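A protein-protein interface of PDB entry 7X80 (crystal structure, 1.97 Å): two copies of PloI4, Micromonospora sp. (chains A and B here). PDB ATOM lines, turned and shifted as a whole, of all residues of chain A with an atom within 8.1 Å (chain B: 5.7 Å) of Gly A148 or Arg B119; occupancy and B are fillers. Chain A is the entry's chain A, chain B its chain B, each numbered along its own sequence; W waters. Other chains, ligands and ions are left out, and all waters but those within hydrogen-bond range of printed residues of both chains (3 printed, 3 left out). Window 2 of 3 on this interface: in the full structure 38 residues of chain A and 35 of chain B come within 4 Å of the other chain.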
ATOM      1  N   SER A   2      -8.888 -16.644 -27.637  1.00  0.00           N
ATOM      2  CA  SER A   2     -10.147 -16.332 -26.979  1.00  0.00           C
ATOM      3  C   SER A   2     -10.529 -17.431 -25.990  1.00  0.00           C
ATOM      4  O   SER A   2      -9.886 -18.484 -25.892  1.00  0.00           O
ATOM      5  CB  SER A   2     -11.265 -16.158 -27.984  1.00  0.00           C
ATOM      6  OG  SER A   2     -11.535 -17.412 -28.562  1.00  0.00           O
ATOM      7  N   HIS A   3     -11.611 -17.184 -25.257  1.00  0.00           N
ATOM      8  CA  HIS A   3     -12.075 -18.110 -24.232  1.00  0.00           C
ATOM      9  C   HIS A   3     -12.910 -19.219 -24.844  1.00  0.00           C
ATOM     10  O   HIS A   3     -13.850 -18.955 -25.605  1.00  0.00           O
ATOM     11  CB  HIS A   3     -12.935 -17.422 -23.182  1.00  0.00           C
ATOM     12  CG  HIS A   3     -12.963 -18.150 -21.876  1.00  0.00           C
ATOM     13  ND1 HIS A   3     -14.011 -18.050 -20.982  1.00  0.00           N
ATOM     14  CD2 HIS A   3     -12.017 -18.902 -21.262  1.00  0.00           C
ATOM     15  CE1 HIS A   3     -13.736 -18.762 -19.904  1.00  0.00           C
ATOM     16  NE2 HIS A   3     -12.528 -19.280 -20.043  1.00  0.00           N
ATOM     17  N   MET A   4     -12.618 -20.454 -24.458  1.00  0.00           N
ATOM     18  CA  MET A   4     -13.337 -21.604 -24.983  1.00  0.00           C
ATOM     19  C   MET A   4     -14.327 -22.189 -23.987  1.00  0.00           C
ATOM     20  O   MET A   4     -15.257 -22.891 -24.395  1.00  0.00           O
ATOM     21  CB  MET A   4     -12.346 -22.691 -25.412  1.00  0.00           C
ATOM     22  CG  MET A   4     -11.641 -22.363 -26.724  1.00  0.00           C
ATOM     23  SD  MET A   4     -12.655 -22.672 -28.179  1.00  0.00           S
ATOM     24  CE  MET A   4     -12.727 -24.459 -28.133  1.00  0.00           C
ATOM     25  N   SER A   5     -14.150 -21.917 -22.696  1.00  0.00           N
ATOM     26  CA  SER A   5     -15.097 -22.395 -21.699  1.00  0.00           C
ATOM     27  C   SER A   5     -16.466 -21.776 -21.941  1.00  0.00           C
ATOM     28  O   SER A   5     -16.589 -20.577 -22.206  1.00  0.00           O
ATOM     29  CB  SER A   5     -14.614 -22.059 -20.286  1.00  0.00           C
ATOM     30  OG  SER A   5     -15.680 -22.159 -19.354  1.00  0.00           O
ATOM     31  N   THR A   6     -17.500 -22.604 -21.866  1.00  0.00           N
ATOM     32  CA  THR A   6     -18.886 -22.176 -22.064  1.00  0.00           C
ATOM     33  C   THR A   6     -19.764 -22.708 -20.928  1.00  0.00           C
ATOM     34  O   THR A   6     -20.860 -23.247 -21.131  1.00  0.00           O
ATOM     35  CB  THR A   6     -19.380 -22.623 -23.437  1.00  0.00           C
ATOM     36  OG1 THR A   6     -19.465 -24.053 -23.471  1.00  0.00           O
ATOM     37  CG2 THR A   6     -18.422 -22.153 -24.529  1.00  0.00           C
ATOM     38  N   VAL A   7     -19.250 -22.528 -19.702  1.00  0.00           N
ATOM     39  CA  VAL A   7     -19.888 -23.002 -18.475  1.00  0.00           C
ATOM     40  C   VAL A   7     -21.229 -22.307 -18.241  1.00  0.00           C
ATOM     41  O   VAL A   7     -22.224 -22.947 -17.875  1.00  0.00           O
ATOM     42  CB  VAL A   7     -18.914 -22.779 -17.300  1.00  0.00           C
ATOM     43  CG1 VAL A   7     -19.620 -22.800 -15.962  1.00  0.00           C
ATOM     44  CG2 VAL A   7     -17.789 -23.811 -17.349  1.00  0.00           C
ATOM     45  N   THR A   8     -21.271 -20.989 -18.428  1.00  0.00           N
ATOM     46  CA  THR A   8     -22.472 -20.176 -18.280  1.00  0.00           C
ATOM     47  C   THR A   8     -22.896 -19.671 -19.655  1.00  0.00           C
ATOM     48  O   THR A   8     -22.047 -19.259 -20.449  1.00  0.00           O
ATOM     49  CB  THR A   8     -22.201 -18.991 -17.357  1.00  0.00           C
ATOM     50  OG1 THR A   8     -21.901 -19.476 -16.047  1.00  0.00           O
ATOM     51  CG2 THR A   8     -23.400 -18.048 -17.295  1.00  0.00           C
ATOM     52  N   THR A   9     -24.196 -19.716 -19.945  1.00  0.00           N
ATOM     53  CA  THR A   9     -24.714 -19.255 -21.228  1.00  0.00           C
ATOM     54  C   THR A   9     -25.754 -18.170 -21.001  1.00  0.00           C
ATOM     55  O   THR A   9     -26.593 -18.282 -20.100  1.00  0.00           O
ATOM     56  CB  THR A   9     -25.332 -20.411 -22.049  1.00  0.00           C
ATOM     57  OG1 THR A   9     -24.287 -21.248 -22.564  1.00  0.00           O
ATOM     58  CG2 THR A   9     -26.155 -19.870 -23.256  1.00  0.00           C
ATOM     59  N   ILE A  10     -25.673 -17.109 -21.800  1.00  0.00           N
ATOM     60  CA  ILE A  10     -26.749 -16.135 -21.940  1.00  0.00           C
ATOM     61  C   ILE A  10     -27.144 -16.121 -23.406  1.00  0.00           C
ATOM     62  O   ILE A  10     -26.311 -15.838 -24.280  1.00  0.00           O
ATOM     63  CB  ILE A  10     -26.339 -14.732 -21.474  1.00  0.00           C
ATOM     64  CG1 ILE A  10     -26.025 -14.748 -19.977  1.00  0.00           C
ATOM     65  CG2 ILE A  10     -27.493 -13.752 -21.750  1.00  0.00           C
ATOM     66  CD1 ILE A  10     -25.683 -13.392 -19.427  1.00  0.00           C
ATOM     67  N   GLY A 113     -19.234  -9.256 -22.744  1.00  0.00           N
ATOM     68  CA  GLY A 113     -19.930  -8.796 -21.558  1.00  0.00           C
ATOM     69  C   GLY A 113     -18.951  -8.078 -20.656  1.00  0.00           C
ATOM     70  O   GLY A 113     -17.898  -8.624 -20.305  1.00  0.00           O
ATOM     71  N   TYR A 118     -23.406 -10.008 -17.406  1.00  0.00           N
ATOM     72  CA  TYR A 118     -22.675 -10.314 -18.635  1.00  0.00           C
ATOM     73  C   TYR A 118     -21.160 -10.348 -18.444  1.00  0.00           C
ATOM     74  O   TYR A 118     -20.467 -10.900 -19.300  1.00  0.00           O
ATOM     75  CB  TYR A 118     -23.042  -9.280 -19.724  1.00  0.00           C
ATOM     76  CG  TYR A 118     -24.528  -9.042 -19.728  1.00  0.00           C
ATOM     77  CD1 TYR A 118     -25.391  -9.950 -20.332  1.00  0.00           C
ATOM     78  CD2 TYR A 118     -25.073  -7.936 -19.081  1.00  0.00           C
ATOM     79  CE1 TYR A 118     -26.776  -9.768 -20.278  1.00  0.00           C
ATOM     80  CE2 TYR A 118     -26.453  -7.736 -19.026  1.00  0.00           C
ATOM     81  CZ  TYR A 118     -27.301  -8.659 -19.620  1.00  0.00           C
ATOM     82  OH  TYR A 118     -28.671  -8.466 -19.566  1.00  0.00           O
ATOM     83  N   ARG A 119     -20.635  -9.779 -17.353  1.00  0.00           N
ATOM     84  CA  ARG A 119     -19.191  -9.618 -17.195  1.00  0.00           C
ATOM     85  C   ARG A 119     -18.425 -10.923 -17.379  1.00  0.00           C
ATOM     86  O   ARG A 119     -18.736 -11.941 -16.753  1.00  0.00           O
ATOM     87  CB  ARG A 119     -18.861  -9.037 -15.816  1.00  0.00           C
ATOM     88  CG  ARG A 119     -17.377  -8.645 -15.692  1.00  0.00           C
ATOM     89  CD  ARG A 119     -16.959  -8.353 -14.254  1.00  0.00           C
ATOM     90  NE  ARG A 119     -17.550  -7.102 -13.808  1.00  0.00           N
ATOM     91  CZ  ARG A 119     -16.979  -5.907 -13.960  1.00  0.00           C
ATOM     92  NH1 ARG A 119     -17.601  -4.816 -13.524  1.00  0.00           N
ATOM     93  NH2 ARG A 119     -15.786  -5.800 -14.546  1.00  0.00           N
ATOM     94  N   GLY A 120     -17.383 -10.873 -18.209  1.00  0.00           N
ATOM     95  CA  GLY A 120     -16.535 -12.028 -18.418  1.00  0.00           C
ATOM     96  C   GLY A 120     -17.042 -13.037 -19.428  1.00  0.00           C
ATOM     97  O   GLY A 120     -16.329 -14.005 -19.722  1.00  0.00           O
ATOM     98  N   LEU A 121     -18.237 -12.850 -19.974  1.00  0.00           N
ATOM     99  CA  LEU A 121     -18.737 -13.727 -21.021  1.00  0.00           C
ATOM    100  C   LEU A 121     -18.445 -13.098 -22.377  1.00  0.00           C
ATOM    101  O   LEU A 121     -18.296 -11.880 -22.495  1.00  0.00           O
ATOM    102  CB  LEU A 121     -20.240 -13.982 -20.867  1.00  0.00           C
ATOM    103  CG  LEU A 121     -20.684 -14.369 -19.457  1.00  0.00           C
ATOM    104  CD1 LEU A 121     -22.177 -14.675 -19.422  1.00  0.00           C
ATOM    105  CD2 LEU A 121     -19.871 -15.553 -18.975  1.00  0.00           C
ATOM    106  N   SER A 122     -18.376 -13.945 -23.397  1.00  0.00           N
ATOM    107  CA  SER A 122     -18.032 -13.515 -24.751  1.00  0.00           C
ATOM    108  C   SER A 122     -18.826 -14.333 -25.759  1.00  0.00           C
ATOM    109  O   SER A 122     -19.294 -15.437 -25.473  1.00  0.00           O
ATOM    110  CB  SER A 122     -16.529 -13.673 -25.025  1.00  0.00           C
ATOM    111  OG  SER A 122     -16.134 -15.014 -24.777  1.00  0.00           O
ATOM    112  N   GLY A 123     -18.977 -13.781 -26.954  1.00  0.00           N
ATOM    113  CA  GLY A 123     -19.735 -14.486 -27.961  1.00  0.00           C
ATOM    114  C   GLY A 123     -20.002 -13.592 -29.150  1.00  0.00           C
ATOM    115  O   GLY A 123     -19.077 -12.954 -29.661  1.00  0.00           O
ATOM    116  N   VAL A 145     -25.553 -13.940 -28.076  1.00  0.00           N
ATOM    117  CA  VAL A 145     -25.193 -15.200 -27.441  1.00  0.00           C
ATOM    118  C   VAL A 145     -23.865 -14.987 -26.749  1.00  0.00           C
ATOM    119  O   VAL A 145     -22.882 -14.614 -27.397  1.00  0.00           O
ATOM    120  CB  VAL A 145     -25.100 -16.354 -28.456  1.00  0.00           C
ATOM    121  CG1 VAL A 145     -25.000 -17.684 -27.734  1.00  0.00           C
ATOM    122  CG2 VAL A 145     -26.290 -16.328 -29.390  1.00  0.00           C
ATOM    123  N   LEU A 146     -23.826 -15.212 -25.440  1.00  0.00           N
ATOM    124  CA  LEU A 146     -22.602 -15.078 -24.666  1.00  0.00           C
ATOM    125  C   LEU A 146     -22.400 -16.331 -23.837  1.00  0.00           C
ATOM    126  O   LEU A 146     -23.365 -16.913 -23.318  1.00  0.00           O
ATOM    127  CB  LEU A 146     -22.629 -13.869 -23.720  1.00  0.00           C
ATOM    128  CG  LEU A 146     -22.822 -12.481 -24.323  1.00  0.00           C
ATOM    129  CD1 LEU A 146     -23.111 -11.478 -23.206  1.00  0.00           C
ATOM    130  CD2 LEU A 146     -21.592 -12.071 -25.113  1.00  0.00           C
ATOM    131  N   ASN A 147     -21.141 -16.721 -23.689  1.00  0.00           N
ATOM    132  CA  ASN A 147     -20.812 -17.819 -22.795  1.00  0.00           C
ATOM    133  C   ASN A 147     -19.432 -17.571 -22.206  1.00  0.00           C
ATOM    134  O   ASN A 147     -18.667 -16.732 -22.688  1.00  0.00           O
ATOM    135  CB  ASN A 147     -20.867 -19.178 -23.501  1.00  0.00           C
ATOM    136  CG  ASN A 147     -20.193 -19.153 -24.851  1.00  0.00           C
ATOM    137  OD1 ASN A 147     -19.113 -18.576 -25.022  1.00  0.00           O
ATOM    138  ND2 ASN A 147     -20.845 -19.754 -25.834  1.00  0.00           N
ATOM    139  N   GLY A 148     -19.146 -18.286 -21.132  1.00  0.00           N
ATOM    140  CA  GLY A 148     -17.874 -18.115 -20.470  1.00  0.00           C
ATOM    141  C   GLY A 148     -17.793 -18.896 -19.187  1.00  0.00           C
ATOM    142  O   GLY A 148     -16.704 -18.989 -18.611  1.00  0.00           O
ATOM    143  OXT GLY A 148     -18.813 -19.427 -18.733  1.00  0.00           O
ATOM    144  N   GLY B  89      -1.283 -12.708 -20.456  1.00  0.00           N
ATOM    145  CA  GLY B  89      -2.536 -12.207 -19.904  1.00  0.00           C
ATOM    146  C   GLY B  89      -3.831 -12.718 -20.515  1.00  0.00           C
ATOM    147  O   GLY B  89      -4.861 -12.750 -19.827  1.00  0.00           O
ATOM    148  N   GLY B 113     -11.082  -7.123 -21.366  1.00  0.00           N
ATOM    149  CA  GLY B 113     -10.389  -8.400 -21.267  1.00  0.00           C
ATOM    150  C   GLY B 113     -11.412  -9.517 -21.356  1.00  0.00           C
ATOM    151  O   GLY B 113     -12.452  -9.464 -20.687  1.00  0.00           O
ATOM    152  N   VAL B 114     -11.131 -10.535 -22.182  1.00  0.00           N
ATOM    153  CA  VAL B 114     -12.114 -11.582 -22.443  1.00  0.00           C
ATOM    154  C   VAL B 114     -11.604 -12.994 -22.201  1.00  0.00           C
ATOM    155  O   VAL B 114     -12.378 -13.942 -22.351  1.00  0.00           O
ATOM    156  CB  VAL B 114     -12.695 -11.480 -23.867  1.00  0.00           C
ATOM    157  CG1 VAL B 114     -13.416 -10.160 -24.032  1.00  0.00           C
ATOM    158  CG2 VAL B 114     -11.602 -11.697 -24.926  1.00  0.00           C
ATOM    159  N   SER B 115     -10.338 -13.186 -21.835  1.00  0.00           N
ATOM    160  CA  SER B 115      -9.819 -14.537 -21.629  1.00  0.00           C
ATOM    161  C   SER B 115      -8.578 -14.459 -20.753  1.00  0.00           C
ATOM    162  O   SER B 115      -8.040 -13.379 -20.494  1.00  0.00           O
ATOM    163  CB  SER B 115      -9.510 -15.265 -22.954  1.00  0.00           C
ATOM    164  OG  SER B 115      -8.376 -14.725 -23.632  1.00  0.00           O
ATOM    165  N   GLY B 116      -8.142 -15.628 -20.284  1.00  0.00           N
ATOM    166  CA  GLY B 116      -6.982 -15.695 -19.409  1.00  0.00           C
ATOM    167  C   GLY B 116      -7.213 -14.883 -18.151  1.00  0.00           C
ATOM    168  O   GLY B 116      -8.352 -14.660 -17.714  1.00  0.00           O
ATOM    169  N   ARG B 117      -6.119 -14.402 -17.565  1.00  0.00           N
ATOM    170  CA  ARG B 117      -6.202 -13.601 -16.350  1.00  0.00           C
ATOM    171  C   ARG B 117      -6.799 -12.223 -16.596  1.00  0.00           C
ATOM    172  O   ARG B 117      -7.069 -11.500 -15.633  1.00  0.00           O
ATOM    173  CB  ARG B 117      -4.812 -13.488 -15.702  1.00  0.00           C
ATOM    174  CG  ARG B 117      -3.863 -12.492 -16.360  1.00  0.00           C
ATOM    175  CD  ARG B 117      -2.438 -12.582 -15.772  1.00  0.00           C
ATOM    176  NE  ARG B 117      -1.578 -11.510 -16.272  1.00  0.00           N
ATOM    177  CZ  ARG B 117      -1.248 -10.425 -15.580  1.00  0.00           C
ATOM    178  NH1 ARG B 117      -1.685 -10.272 -14.337  1.00  0.00           N
ATOM    179  NH2 ARG B 117      -0.471  -9.498 -16.131  1.00  0.00           N
ATOM    180  N   TYR B 118      -7.029 -11.844 -17.850  1.00  0.00           N
ATOM    181  CA  TYR B 118      -7.576 -10.528 -18.117  1.00  0.00           C
ATOM    182  C   TYR B 118      -9.106 -10.539 -18.178  1.00  0.00           C
ATOM    183  O   TYR B 118      -9.717  -9.467 -18.252  1.00  0.00           O
ATOM    184  CB  TYR B 118      -7.017  -9.992 -19.448  1.00  0.00           C
ATOM    185  CG  TYR B 118      -5.583  -9.538 -19.315  1.00  0.00           C
ATOM    186  CD1 TYR B 118      -5.031  -9.348 -18.066  1.00  0.00           C
ATOM    187  CD2 TYR B 118      -4.786  -9.290 -20.423  1.00  0.00           C
ATOM    188  CE1 TYR B 118      -3.718  -8.963 -17.913  1.00  0.00           C
ATOM    189  CE2 TYR B 118      -3.464  -8.874 -20.277  1.00  0.00           C
ATOM    190  CZ  TYR B 118      -2.940  -8.707 -19.007  1.00  0.00           C
ATOM    191  OH  TYR B 118      -1.638  -8.303 -18.779  1.00  0.00           O
ATOM    192  N   ARG B 119      -9.728 -11.723 -18.145  1.00  0.00           N
ATOM    193  CA  ARG B 119     -11.171 -11.860 -18.340  1.00  0.00           C
ATOM    194  C   ARG B 119     -11.970 -11.001 -17.355  1.00  0.00           C
ATOM    195  O   ARG B 119     -11.760 -11.067 -16.145  1.00  0.00           O
ATOM    196  CB  ARG B 119     -11.574 -13.333 -18.183  1.00  0.00           C
ATOM    197  CG  ARG B 119     -13.023 -13.691 -18.597  1.00  0.00           C
ATOM    198  CD  ARG B 119     -13.120 -15.133 -19.125  1.00  0.00           C
ATOM    199  NE  ARG B 119     -13.242 -16.103 -18.037  1.00  0.00           N
ATOM    200  CZ  ARG B 119     -14.379 -16.423 -17.421  1.00  0.00           C
ATOM    201  NH1 ARG B 119     -15.537 -15.879 -17.799  1.00  0.00           N
ATOM    202  NH2 ARG B 119     -14.364 -17.311 -16.433  1.00  0.00           N
ATOM    203  N   GLY B 120     -12.942 -10.265 -17.886  1.00  0.00           N
ATOM    204  CA  GLY B 120     -13.871  -9.570 -17.033  1.00  0.00           C
ATOM    205  C   GLY B 120     -13.358  -8.272 -16.479  1.00  0.00           C
ATOM    206  O   GLY B 120     -14.073  -7.629 -15.703  1.00  0.00           O
ATOM    207  N   LEU B 121     -12.138  -7.872 -16.831  1.00  0.00           N
ATOM    208  CA  LEU B 121     -11.656  -6.535 -16.533  1.00  0.00           C
ATOM    209  C   LEU B 121     -11.873  -5.663 -17.763  1.00  0.00           C
ATOM    210  O   LEU B 121     -11.875  -6.155 -18.887  1.00  0.00           O
ATOM    211  CB  LEU B 121     -10.180  -6.565 -16.158  1.00  0.00           C
ATOM    212  CG  LEU B 121      -9.744  -7.690 -15.219  1.00  0.00           C
ATOM    213  CD1 LEU B 121      -8.227  -7.638 -15.031  1.00  0.00           C
ATOM    214  CD2 LEU B 121     -10.462  -7.536 -13.889  1.00  0.00           C
HETATM  215  O   HOH W   1      -9.218 -18.613 -20.781  1.00  0.00           O
HETATM  216  O   HOH W   2     -15.511  -9.750 -20.484  1.00  0.00           O
HETATM  217  O   HOH W   3     -15.320  -5.812 -17.554  1.00  0.00           O
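Water W2 lies within hydrogen-bond range of the backbone carbonyl oxygen (O) of Gly A113, the backbone carbonyl oxygen (O) of Gly B113 and the backbone NH (N) of Gly A120.
Water W3 lies within hydrogen-bond range of the backbone carbonyl oxygen (O) of Gly B120 (2.9 Å) and the guanidinium group (NH2) of Arg A119 (3.0 Å).
Water W1 bridges the backbone NH of Gly B116 and a ring nitrogen (NE2) of His A3.
The backbone carbonyl oxygen (O) of Gly A120 sits at hydrogen-bond distance from the guanidinium group (NH1) of Arg B119 (2.8 Å).
The chain-end carboxylate of Gly A148 is in salt-bridge range of the guanidinium group of Arg B119 (3.4 Å).
The guanidinium group (NH2) of Arg A119 lies within hydrogen-bond range of the backbone carbonyl oxygen (O) of Gly B120 (2.8 Å).
Ser A2 touches Ser B115.
His A3 touches Val B114 (CB to O, 3.6 Å).
Ser B115 touches His A3.
CE1 of His A3 touches NE of Arg B119 (3.3 Å).
Gly B120 touches Gly A120.
Arg A119 touches Gly B120, and with the chains exchanged Gly A120 touches Arg B119.
Gly A120 touches its own counterpart, Gly B120.
Of the printed residues of chain B, Gly A148 touches Arg B119 (3.4 Å).
Printed residues of chain A within 4 Å of Arg B119: His A3, Gly A120 and Gly A148.
Of the printed residues of chain B, His A3 touches Val B114, Ser B115 and Arg B119.
Printed residues of chain B within 4 Å of Gly A120: Arg B119 (2.8 Å) and Gly B120 (3.9 Å).
Printed residues of chain B within 4 Å of Arg A119: Gly B120.
Of the printed residues of chain A, Val B114 touches His A3 (3.6 Å).
Ile A10 touches none of the printed residues of chain B.
The nearest printed residue of chain B that does not touch Gly A148 is Val B114 (7.2 Å).
The nearest printed residue of chain A that does not touch Arg B119 is Leu A121 (4.5 Å).
The nearest printed residue of chain A that does not touch Ser B115 is Met A4 (6.2 Å).
O of Gly B113 sits at hydrogen-bond distance from N of Gly B120 (3.0 Å).
O of Gly A113 is in hydrogen-bond range of N of Gly A120, 3.1 Å away.
The backbone NH (N) of Thr A8 is in hydrogen-bond range of the chain-end carboxylate (OXT) of Gly A148.
O of Gly A148 lies within hydrogen-bond range of OG of Ser A5, at 3.4 Å.
The backbone NH (N) of Val A7 is in hydrogen-bond range of the chain-end carboxylate (OXT) of Gly A148 (3.3 Å).
Of the 10 printed residues of chain B, 4 touch a printed residue of chain A.
Of the 20 printed residues of chain A, 5 touch a printed residue of chain B.
Among the printed residues, no Asp or Glu carboxylate lies within 4 Å of a Lys or Arg side-chain nitrogen of the other chain.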
